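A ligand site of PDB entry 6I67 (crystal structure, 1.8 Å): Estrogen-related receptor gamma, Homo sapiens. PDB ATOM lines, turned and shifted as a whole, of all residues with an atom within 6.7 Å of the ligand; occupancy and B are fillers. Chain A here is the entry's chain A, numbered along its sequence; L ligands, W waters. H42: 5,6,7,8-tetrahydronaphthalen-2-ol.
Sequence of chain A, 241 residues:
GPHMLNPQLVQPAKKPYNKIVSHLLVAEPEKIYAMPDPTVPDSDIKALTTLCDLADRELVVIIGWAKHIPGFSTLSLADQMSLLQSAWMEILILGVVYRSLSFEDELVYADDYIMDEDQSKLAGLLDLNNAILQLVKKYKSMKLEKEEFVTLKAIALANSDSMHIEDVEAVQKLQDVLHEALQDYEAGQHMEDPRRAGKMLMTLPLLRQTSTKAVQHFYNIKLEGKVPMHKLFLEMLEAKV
The guanidinium group (NH2) of Arg 99 sits at hydrogen-bond distance from an oxygen (OAA) of the ligand, 3.2 Å away. OE1 of Glu 58 sits at hydrogen-bond distance from OAA of the ligand (2.4 Å).
Water W1 lies within hydrogen-bond range of OE2 of Glu 58, O of Leu 92, OAA of the ligand and NH1 of Arg 99.
NH1 of Arg 99 sits close to O of Gly 95 (3.5 Å). NE of Arg 99 is in hydrogen-bond range of O of Val 108, 3.0 Å away. OH of Tyr 109 lies within hydrogen-bond range of OD1 of Asn 129 (2.7 Å). The backbone carbonyl oxygen (O) of Tyr 109 sits at hydrogen-bond distance from the guanidinium group (NH2) of Arg 99 (3.0 Å). The guanidinium group (NH2) of Arg 99 lies within salt-bridge range of the side-chain carboxylate (OE1) of Glu 58, 3.9 Å away.
Leu 51 touches the ligand. Leu 54 touches the ligand (CD2 to CAB, 3.8 Å). CB of Ala 55 touches CAC of the ligand (3.7 Å). Met 89 touches the ligand. Leu 92 touches the ligand. Val 96 touches the ligand. CE1 of Tyr 109 touches CAK of the ligand (3.5 Å). Phe 218 touches the ligand. Hydrophobic or aromatic side chains within 4 Å of the ligand: Leu 54, Ala 55, Met 89, Leu 92, Val 96, Tyr 109 and Phe 218. Ten residues have an atom within 4 Å of the ligand: Leu 51, Leu 54, Ala 55, Glu 58, Met 89, Leu 92, Val 96, Arg 99, Tyr 109 and Phe 218. The nearest printed residue that does not touch the ligand is Ile 93 (4.2 Å).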
ATOM      1  N   THR A  50     -19.857   5.877  11.428  1.00  0.00           N
ATOM      2  CA  THR A  50     -20.480   7.155  11.732  1.00  0.00           C
ATOM      3  C   THR A  50     -20.497   7.406  13.238  1.00  0.00           C
ATOM      4  O   THR A  50     -20.207   8.512  13.706  1.00  0.00           O
ATOM      5  CB  THR A  50     -21.904   7.202  11.179  1.00  0.00           C
ATOM      6  OG1 THR A  50     -21.872   7.004   9.756  1.00  0.00           O
ATOM      7  CG2 THR A  50     -22.581   8.540  11.490  1.00  0.00           C
ATOM      8  N   LEU A  51     -20.885   6.385  13.991  1.00  0.00           N
ATOM      9  CA  LEU A  51     -20.982   6.527  15.447  1.00  0.00           C
ATOM     10  C   LEU A  51     -19.625   6.734  16.082  1.00  0.00           C
ATOM     11  O   LEU A  51     -19.481   7.560  16.993  1.00  0.00           O
ATOM     12  CB  LEU A  51     -21.669   5.292  16.028  1.00  0.00           C
ATOM     13  CG  LEU A  51     -23.167   5.234  15.758  1.00  0.00           C
ATOM     14  CD1 LEU A  51     -23.723   3.940  16.287  1.00  0.00           C
ATOM     15  CD2 LEU A  51     -23.926   6.425  16.358  1.00  0.00           C
ATOM     16  N   CYS A  52     -18.617   5.969  15.660  1.00  0.00           N
ATOM     17  CA  CYS A  52     -17.287   6.115  16.235  1.00  0.00           C
ATOM     18  C   CYS A  52     -16.672   7.452  15.878  1.00  0.00           C
ATOM     19  O   CYS A  52     -15.938   8.027  16.685  1.00  0.00           O
ATOM     20  CB  CYS A  52     -16.373   4.985  15.788  1.00  0.00           C
ATOM     21  SG  CYS A  52     -16.877   3.407  16.462  1.00  0.00           S
ATOM     22  N   LEU A  54     -18.461  10.221  15.346  1.00  0.00           N
ATOM     23  CA  LEU A  54     -19.190  11.180  16.176  1.00  0.00           C
ATOM     24  C   LEU A  54     -18.676  11.165  17.605  1.00  0.00           C
ATOM     25  O   LEU A  54     -18.443  12.228  18.205  1.00  0.00           O
ATOM     26  CB  LEU A  54     -20.680  10.851  16.144  1.00  0.00           C
ATOM     27  CG  LEU A  54     -21.604  11.662  17.029  1.00  0.00           C
ATOM     28  CD1 LEU A  54     -21.656  13.145  16.614  1.00  0.00           C
ATOM     29  CD2 LEU A  54     -22.997  11.047  17.037  1.00  0.00           C
ATOM     30  N   ALA A  55     -18.471   9.976  18.172  1.00  0.00           N
ATOM     31  CA  ALA A  55     -17.946   9.878  19.541  1.00  0.00           C
ATOM     32  C   ALA A  55     -16.571  10.513  19.653  1.00  0.00           C
ATOM     33  O   ALA A  55     -16.270  11.186  20.643  1.00  0.00           O
ATOM     34  CB  ALA A  55     -17.896   8.419  19.973  1.00  0.00           C
ATOM     35  N   ASP A  56     -15.721  10.304  18.643  1.00  0.00           N
ATOM     36  CA  ASP A  56     -14.392  10.913  18.671  1.00  0.00           C
ATOM     37  C   ASP A  56     -14.481  12.434  18.769  1.00  0.00           C
ATOM     38  O   ASP A  56     -13.756  13.050  19.551  1.00  0.00           O
ATOM     39  CB  ASP A  56     -13.598  10.498  17.429  1.00  0.00           C
ATOM     40  CG  ASP A  56     -12.145  10.986  17.464  1.00  0.00           C
ATOM     41  OD1 ASP A  56     -11.296  10.337  18.101  1.00  0.00           O
ATOM     42  OD2 ASP A  56     -11.852  12.035  16.846  1.00  0.00           O
ATOM     43  N   GLU A  58     -17.101  14.168  19.876  1.00  0.00           N
ATOM     44  CA  GLU A  58     -17.684  14.502  21.162  1.00  0.00           C
ATOM     45  C   GLU A  58     -16.659  14.422  22.277  1.00  0.00           C
ATOM     46  O   GLU A  58     -16.726  15.224  23.228  1.00  0.00           O
ATOM     47  CB  GLU A  58     -18.867  13.593  21.476  1.00  0.00           C
ATOM     48  CG  GLU A  58     -20.099  13.843  20.639  1.00  0.00           C
ATOM     49  CD  GLU A  58     -21.343  13.272  21.267  1.00  0.00           C
ATOM     50  OE1 GLU A  58     -22.008  12.472  20.585  1.00  0.00           O
ATOM     51  OE2 GLU A  58     -21.637  13.608  22.439  1.00  0.00           O
ATOM     52  N   TRP A  88     -15.713   8.318  30.218  1.00  0.00           N
ATOM     53  CA  TRP A  88     -16.062   8.943  28.938  1.00  0.00           C
ATOM     54  C   TRP A  88     -17.335   8.343  28.337  1.00  0.00           C
ATOM     55  O   TRP A  88     -18.166   9.073  27.779  1.00  0.00           O
ATOM     56  CB  TRP A  88     -14.895   8.815  27.953  1.00  0.00           C
ATOM     57  CG  TRP A  88     -14.504   7.407  27.634  1.00  0.00           C
ATOM     58  CD1 TRP A  88     -13.743   6.582  28.402  1.00  0.00           C
ATOM     59  CD2 TRP A  88     -14.841   6.669  26.453  1.00  0.00           C
ATOM     60  NE1 TRP A  88     -13.587   5.364  27.773  1.00  0.00           N
ATOM     61  CE2 TRP A  88     -14.250   5.401  26.575  1.00  0.00           C
ATOM     62  CE3 TRP A  88     -15.592   6.967  25.308  1.00  0.00           C
ATOM     63  CZ2 TRP A  88     -14.390   4.412  25.594  1.00  0.00           C
ATOM     64  CZ3 TRP A  88     -15.715   5.990  24.325  1.00  0.00           C
ATOM     65  CH2 TRP A  88     -15.114   4.731  24.475  1.00  0.00           C
ATOM     66  N   MET A  89     -17.495   7.028  28.423  1.00  0.00           N
ATOM     67  CA  MET A  89     -18.663   6.415  27.807  1.00  0.00           C
ATOM     68  C   MET A  89     -19.943   6.705  28.586  1.00  0.00           C
ATOM     69  O   MET A  89     -21.008   6.846  27.993  1.00  0.00           O
ATOM     70  CB  MET A  89     -18.438   4.913  27.645  1.00  0.00           C
ATOM     71  CG  MET A  89     -19.580   4.180  26.981  1.00  0.00           C
ATOM     72  SD  MET A  89     -19.835   4.627  25.232  1.00  0.00           S
ATOM     73  CE  MET A  89     -18.550   3.673  24.428  1.00  0.00           C
ATOM     74  N   ILE A  91     -20.510   9.526  30.006  1.00  0.00           N
ATOM     75  CA  ILE A  91     -20.851  10.877  29.590  1.00  0.00           C
ATOM     76  C   ILE A  91     -21.475  10.865  28.204  1.00  0.00           C
ATOM     77  O   ILE A  91     -22.494  11.534  27.952  1.00  0.00           O
ATOM     78  CB  ILE A  91     -19.605  11.773  29.658  1.00  0.00           C
ATOM     79  CG1 ILE A  91     -19.130  11.893  31.122  1.00  0.00           C
ATOM     80  CG2 ILE A  91     -19.896  13.144  29.043  1.00  0.00           C
ATOM     81  CD1 ILE A  91     -17.703  12.360  31.283  1.00  0.00           C
ATOM     82  N   LEU A  92     -20.896  10.100  27.289  1.00  0.00           N
ATOM     83  CA  LEU A  92     -21.492   9.990  25.954  1.00  0.00           C
ATOM     84  C   LEU A  92     -22.904   9.454  26.034  1.00  0.00           C
ATOM     85  O   LEU A  92     -23.825   9.976  25.389  1.00  0.00           O
ATOM     86  CB  LEU A  92     -20.637   9.067  25.069  1.00  0.00           C
ATOM     87  CG  LEU A  92     -19.292   9.599  24.590  1.00  0.00           C
ATOM     88  CD1 LEU A  92     -18.588   8.525  23.787  1.00  0.00           C
ATOM     89  CD2 LEU A  92     -19.480  10.879  23.767  1.00  0.00           C
ATOM     90  N   ILE A  93     -23.106   8.409  26.836  1.00  0.00           N
ATOM     91  CA  ILE A  93     -24.421   7.780  26.880  1.00  0.00           C
ATOM     92  C   ILE A  93     -25.439   8.704  27.535  1.00  0.00           C
ATOM     93  O   ILE A  93     -26.585   8.785  27.088  1.00  0.00           O
ATOM     94  CB  ILE A  93     -24.326   6.412  27.591  1.00  0.00           C
ATOM     95  CG1 ILE A  93     -23.662   5.409  26.630  1.00  0.00           C
ATOM     96  CG2 ILE A  93     -25.719   5.953  28.023  1.00  0.00           C
ATOM     97  CD1 ILE A  93     -23.398   4.054  27.225  1.00  0.00           C
ATOM     98  N   GLY A  95     -25.576  11.800  27.256  1.00  0.00           N
ATOM     99  CA  GLY A  95     -25.980  12.737  26.222  1.00  0.00           C
ATOM    100  C   GLY A  95     -27.041  12.177  25.297  1.00  0.00           C
ATOM    101  O   GLY A  95     -28.073  12.813  25.050  1.00  0.00           O
ATOM    102  N   VAL A  96     -26.819  10.978  24.771  1.00  0.00           N
ATOM    103  CA  VAL A  96     -27.822  10.365  23.898  1.00  0.00           C
ATOM    104  C   VAL A  96     -29.126  10.192  24.650  1.00  0.00           C
ATOM    105  O   VAL A  96     -30.209  10.422  24.097  1.00  0.00           O
ATOM    106  CB  VAL A  96     -27.325   9.015  23.351  1.00  0.00           C
ATOM    107  CG1 VAL A  96     -28.380   8.409  22.411  1.00  0.00           C
ATOM    108  CG2 VAL A  96     -26.012   9.175  22.661  1.00  0.00           C
ATOM    109  N   ARG A  99     -30.888  13.636  24.958  1.00  0.00           N
ATOM    110  CA  ARG A  99     -31.427  14.088  23.665  1.00  0.00           C
ATOM    111  C   ARG A  99     -32.634  13.278  23.239  1.00  0.00           C
ATOM    112  O   ARG A  99     -33.440  13.771  22.427  1.00  0.00           O
ATOM    113  CB  ARG A  99     -30.334  14.012  22.598  1.00  0.00           C
ATOM    114  CG  ARG A  99     -29.183  14.977  22.836  1.00  0.00           C
ATOM    115  CD  ARG A  99     -28.207  15.006  21.663  1.00  0.00           C
ATOM    116  NE  ARG A  99     -27.450  13.758  21.466  1.00  0.00           N
ATOM    117  CZ  ARG A  99     -26.295  13.474  22.072  1.00  0.00           C
ATOM    118  NH1 ARG A  99     -25.762  14.317  22.950  1.00  0.00           N
ATOM    119  NH2 ARG A  99     -25.668  12.336  21.789  1.00  0.00           N
ATOM    120  N   VAL A 108     -31.502   9.548  19.812  1.00  0.00           N
ATOM    121  CA  VAL A 108     -31.041  10.733  19.072  1.00  0.00           C
ATOM    122  C   VAL A 108     -29.544  10.827  19.337  1.00  0.00           C
ATOM    123  O   VAL A 108     -29.078  11.584  20.192  1.00  0.00           O
ATOM    124  CB  VAL A 108     -31.797  11.998  19.489  1.00  0.00           C
ATOM    125  CG1 VAL A 108     -31.304  13.225  18.681  1.00  0.00           C
ATOM    126  CG2 VAL A 108     -33.298  11.801  19.359  1.00  0.00           C
ATOM    127  N   TYR A 109     -28.767  10.033  18.603  1.00  0.00           N
ATOM    128  CA  TYR A 109     -27.322  10.163  18.706  1.00  0.00           C
ATOM    129  C   TYR A 109     -26.890  11.546  18.256  1.00  0.00           C
ATOM    130  O   TYR A 109     -25.959  12.133  18.824  1.00  0.00           O
ATOM    131  CB  TYR A 109     -26.630   9.068  17.897  1.00  0.00           C
ATOM    132  CG  TYR A 109     -26.533   7.741  18.642  1.00  0.00           C
ATOM    133  CD1 TYR A 109     -25.448   7.474  19.484  1.00  0.00           C
ATOM    134  CD2 TYR A 109     -27.508   6.762  18.514  1.00  0.00           C
ATOM    135  CE1 TYR A 109     -25.352   6.277  20.181  1.00  0.00           C
ATOM    136  CE2 TYR A 109     -27.409   5.544  19.215  1.00  0.00           C
ATOM    137  CZ  TYR A 109     -26.332   5.319  20.041  1.00  0.00           C
ATOM    138  OH  TYR A 109     -26.207   4.129  20.715  1.00  0.00           O
ATOM    139  N   ALA A 110     -27.564  12.083  17.246  1.00  0.00           N
ATOM    140  CA  ALA A 110     -27.424  13.470  16.838  1.00  0.00           C
ATOM    141  C   ALA A 110     -28.715  13.872  16.137  1.00  0.00           C
ATOM    142  O   ALA A 110     -29.537  13.022  15.777  1.00  0.00           O
ATOM    143  CB  ALA A 110     -26.209  13.677  15.916  1.00  0.00           C
ATOM    144  N   LEU A 125     -26.535  -3.295  16.951  1.00  0.00           N
ATOM    145  CA  LEU A 125     -26.594  -2.538  18.201  1.00  0.00           C
ATOM    146  C   LEU A 125     -27.930  -2.676  18.910  1.00  0.00           C
ATOM    147  O   LEU A 125     -28.232  -1.887  19.810  1.00  0.00           O
ATOM    148  CB  LEU A 125     -26.300  -1.055  17.930  1.00  0.00           C
ATOM    149  CG  LEU A 125     -24.870  -0.756  17.486  1.00  0.00           C
ATOM    150  CD1 LEU A 125     -24.688   0.718  17.175  1.00  0.00           C
ATOM    151  CD2 LEU A 125     -23.883  -1.200  18.550  1.00  0.00           C
ATOM    152  N   LEU A 128     -27.417  -3.191  22.824  1.00  0.00           N
ATOM    153  CA  LEU A 128     -26.897  -1.970  23.441  1.00  0.00           C
ATOM    154  C   LEU A 128     -27.948  -0.862  23.436  1.00  0.00           C
ATOM    155  O   LEU A 128     -28.189  -0.216  24.462  1.00  0.00           O
ATOM    156  CB  LEU A 128     -25.619  -1.504  22.733  1.00  0.00           C
ATOM    157  CG  LEU A 128     -25.063  -0.127  23.124  1.00  0.00           C
ATOM    158  CD1 LEU A 128     -24.836  -0.046  24.633  1.00  0.00           C
ATOM    159  CD2 LEU A 128     -23.778   0.180  22.376  1.00  0.00           C
ATOM    160  N   ASN A 129     -28.599  -0.652  22.296  1.00  0.00           N
ATOM    161  CA  ASN A 129     -29.545   0.464  22.221  1.00  0.00           C
ATOM    162  C   ASN A 129     -30.806   0.190  23.024  1.00  0.00           C
ATOM    163  O   ASN A 129     -31.442   1.129  23.525  1.00  0.00           O
ATOM    164  CB  ASN A 129     -29.883   0.762  20.751  1.00  0.00           C
ATOM    165  CG  ASN A 129     -28.809   1.603  20.090  1.00  0.00           C
ATOM    166  OD1 ASN A 129     -27.838   1.979  20.744  1.00  0.00           O
ATOM    167  ND2 ASN A 129     -28.996   1.925  18.807  1.00  0.00           N
ATOM    168  N   ILE A 132     -29.787   1.342  26.424  1.00  0.00           N
ATOM    169  CA  ILE A 132     -29.867   2.794  26.510  1.00  0.00           C
ATOM    170  C   ILE A 132     -31.320   3.253  26.613  1.00  0.00           C
ATOM    171  O   ILE A 132     -31.641   4.189  27.354  1.00  0.00           O
ATOM    172  CB  ILE A 132     -29.141   3.456  25.323  1.00  0.00           C
ATOM    173  CG1 ILE A 132     -27.640   3.104  25.364  1.00  0.00           C
ATOM    174  CG2 ILE A 132     -29.334   4.984  25.348  1.00  0.00           C
ATOM    175  CD1 ILE A 132     -26.897   3.364  24.068  1.00  0.00           C
ATOM    176  N   ALA A 214     -21.399  -0.963  26.389  1.00  0.00           N
ATOM    177  CA  ALA A 214     -20.982  -0.252  25.180  1.00  0.00           C
ATOM    178  C   ALA A 214     -19.477  -0.337  24.973  1.00  0.00           C
ATOM    179  O   ALA A 214     -19.010  -0.521  23.848  1.00  0.00           O
ATOM    180  CB  ALA A 214     -21.433   1.218  25.263  1.00  0.00           C
ATOM    181  N   PHE A 218     -17.788  -2.037  21.596  1.00  0.00           N
ATOM    182  CA  PHE A 218     -16.961  -1.322  20.637  1.00  0.00           C
ATOM    183  C   PHE A 218     -15.490  -1.730  20.708  1.00  0.00           C
ATOM    184  O   PHE A 218     -14.778  -1.580  19.712  1.00  0.00           O
ATOM    185  CB  PHE A 218     -17.129   0.173  20.816  1.00  0.00           C
ATOM    186  CG  PHE A 218     -18.395   0.688  20.219  1.00  0.00           C
ATOM    187  CD1 PHE A 218     -18.412   1.166  18.913  1.00  0.00           C
ATOM    188  CD2 PHE A 218     -19.587   0.641  20.925  1.00  0.00           C
ATOM    189  CE1 PHE A 218     -19.602   1.614  18.339  1.00  0.00           C
ATOM    190  CE2 PHE A 218     -20.779   1.074  20.354  1.00  0.00           C
ATOM    191  CZ  PHE A 218     -20.778   1.567  19.064  1.00  0.00           C
ATOM    192  N   PHE A 233     -10.697   8.432  20.270  1.00  0.00           N
ATOM    193  CA  PHE A 233     -11.631   7.343  20.579  1.00  0.00           C
ATOM    194  C   PHE A 233     -10.886   6.048  20.844  1.00  0.00           C
ATOM    195  O   PHE A 233     -11.216   5.305  21.778  1.00  0.00           O
ATOM    196  CB  PHE A 233     -12.632   7.203  19.421  1.00  0.00           C
ATOM    197  CG  PHE A 233     -13.703   6.145  19.635  1.00  0.00           C
ATOM    198  CD1 PHE A 233     -14.863   6.441  20.343  1.00  0.00           C
ATOM    199  CD2 PHE A 233     -13.574   4.876  19.075  1.00  0.00           C
ATOM    200  CE1 PHE A 233     -15.854   5.487  20.517  1.00  0.00           C
ATOM    201  CE2 PHE A 233     -14.565   3.920  19.238  1.00  0.00           C
ATOM    202  CZ  PHE A 233     -15.702   4.222  19.965  1.00  0.00           C
HETATM  203  CAB H42 L   1     -21.956   9.187  20.168  1.00  0.00           C
HETATM  204  CAC H42 L   1     -21.508   7.926  19.774  1.00  0.00           C
HETATM  205  CAD H42 L   1     -22.764   8.266  22.265  1.00  0.00           C
HETATM  206  CAE H42 L   1     -21.046   4.451  21.403  1.00  0.00           C
HETATM  207  CAF H42 L   1     -22.393   4.444  22.157  1.00  0.00           C
HETATM  208  CAG H42 L   1     -21.323   5.560  20.296  1.00  0.00           C
HETATM  209  CAH H42 L   1     -22.411   5.913  22.672  1.00  0.00           C
HETATM  210  CAI H42 L   1     -22.578   9.355  21.408  1.00  0.00           C
HETATM  211  CAJ H42 L   1     -21.667   6.857  20.657  1.00  0.00           C
HETATM  212  CAK H42 L   1     -22.351   7.013  21.843  1.00  0.00           C
HETATM  213  OAA H42 L   1     -23.016  10.600  21.793  1.00  0.00           O
HETATM  214  O   HOH W   1     -23.333  12.528  24.030  1.00  0.00           O
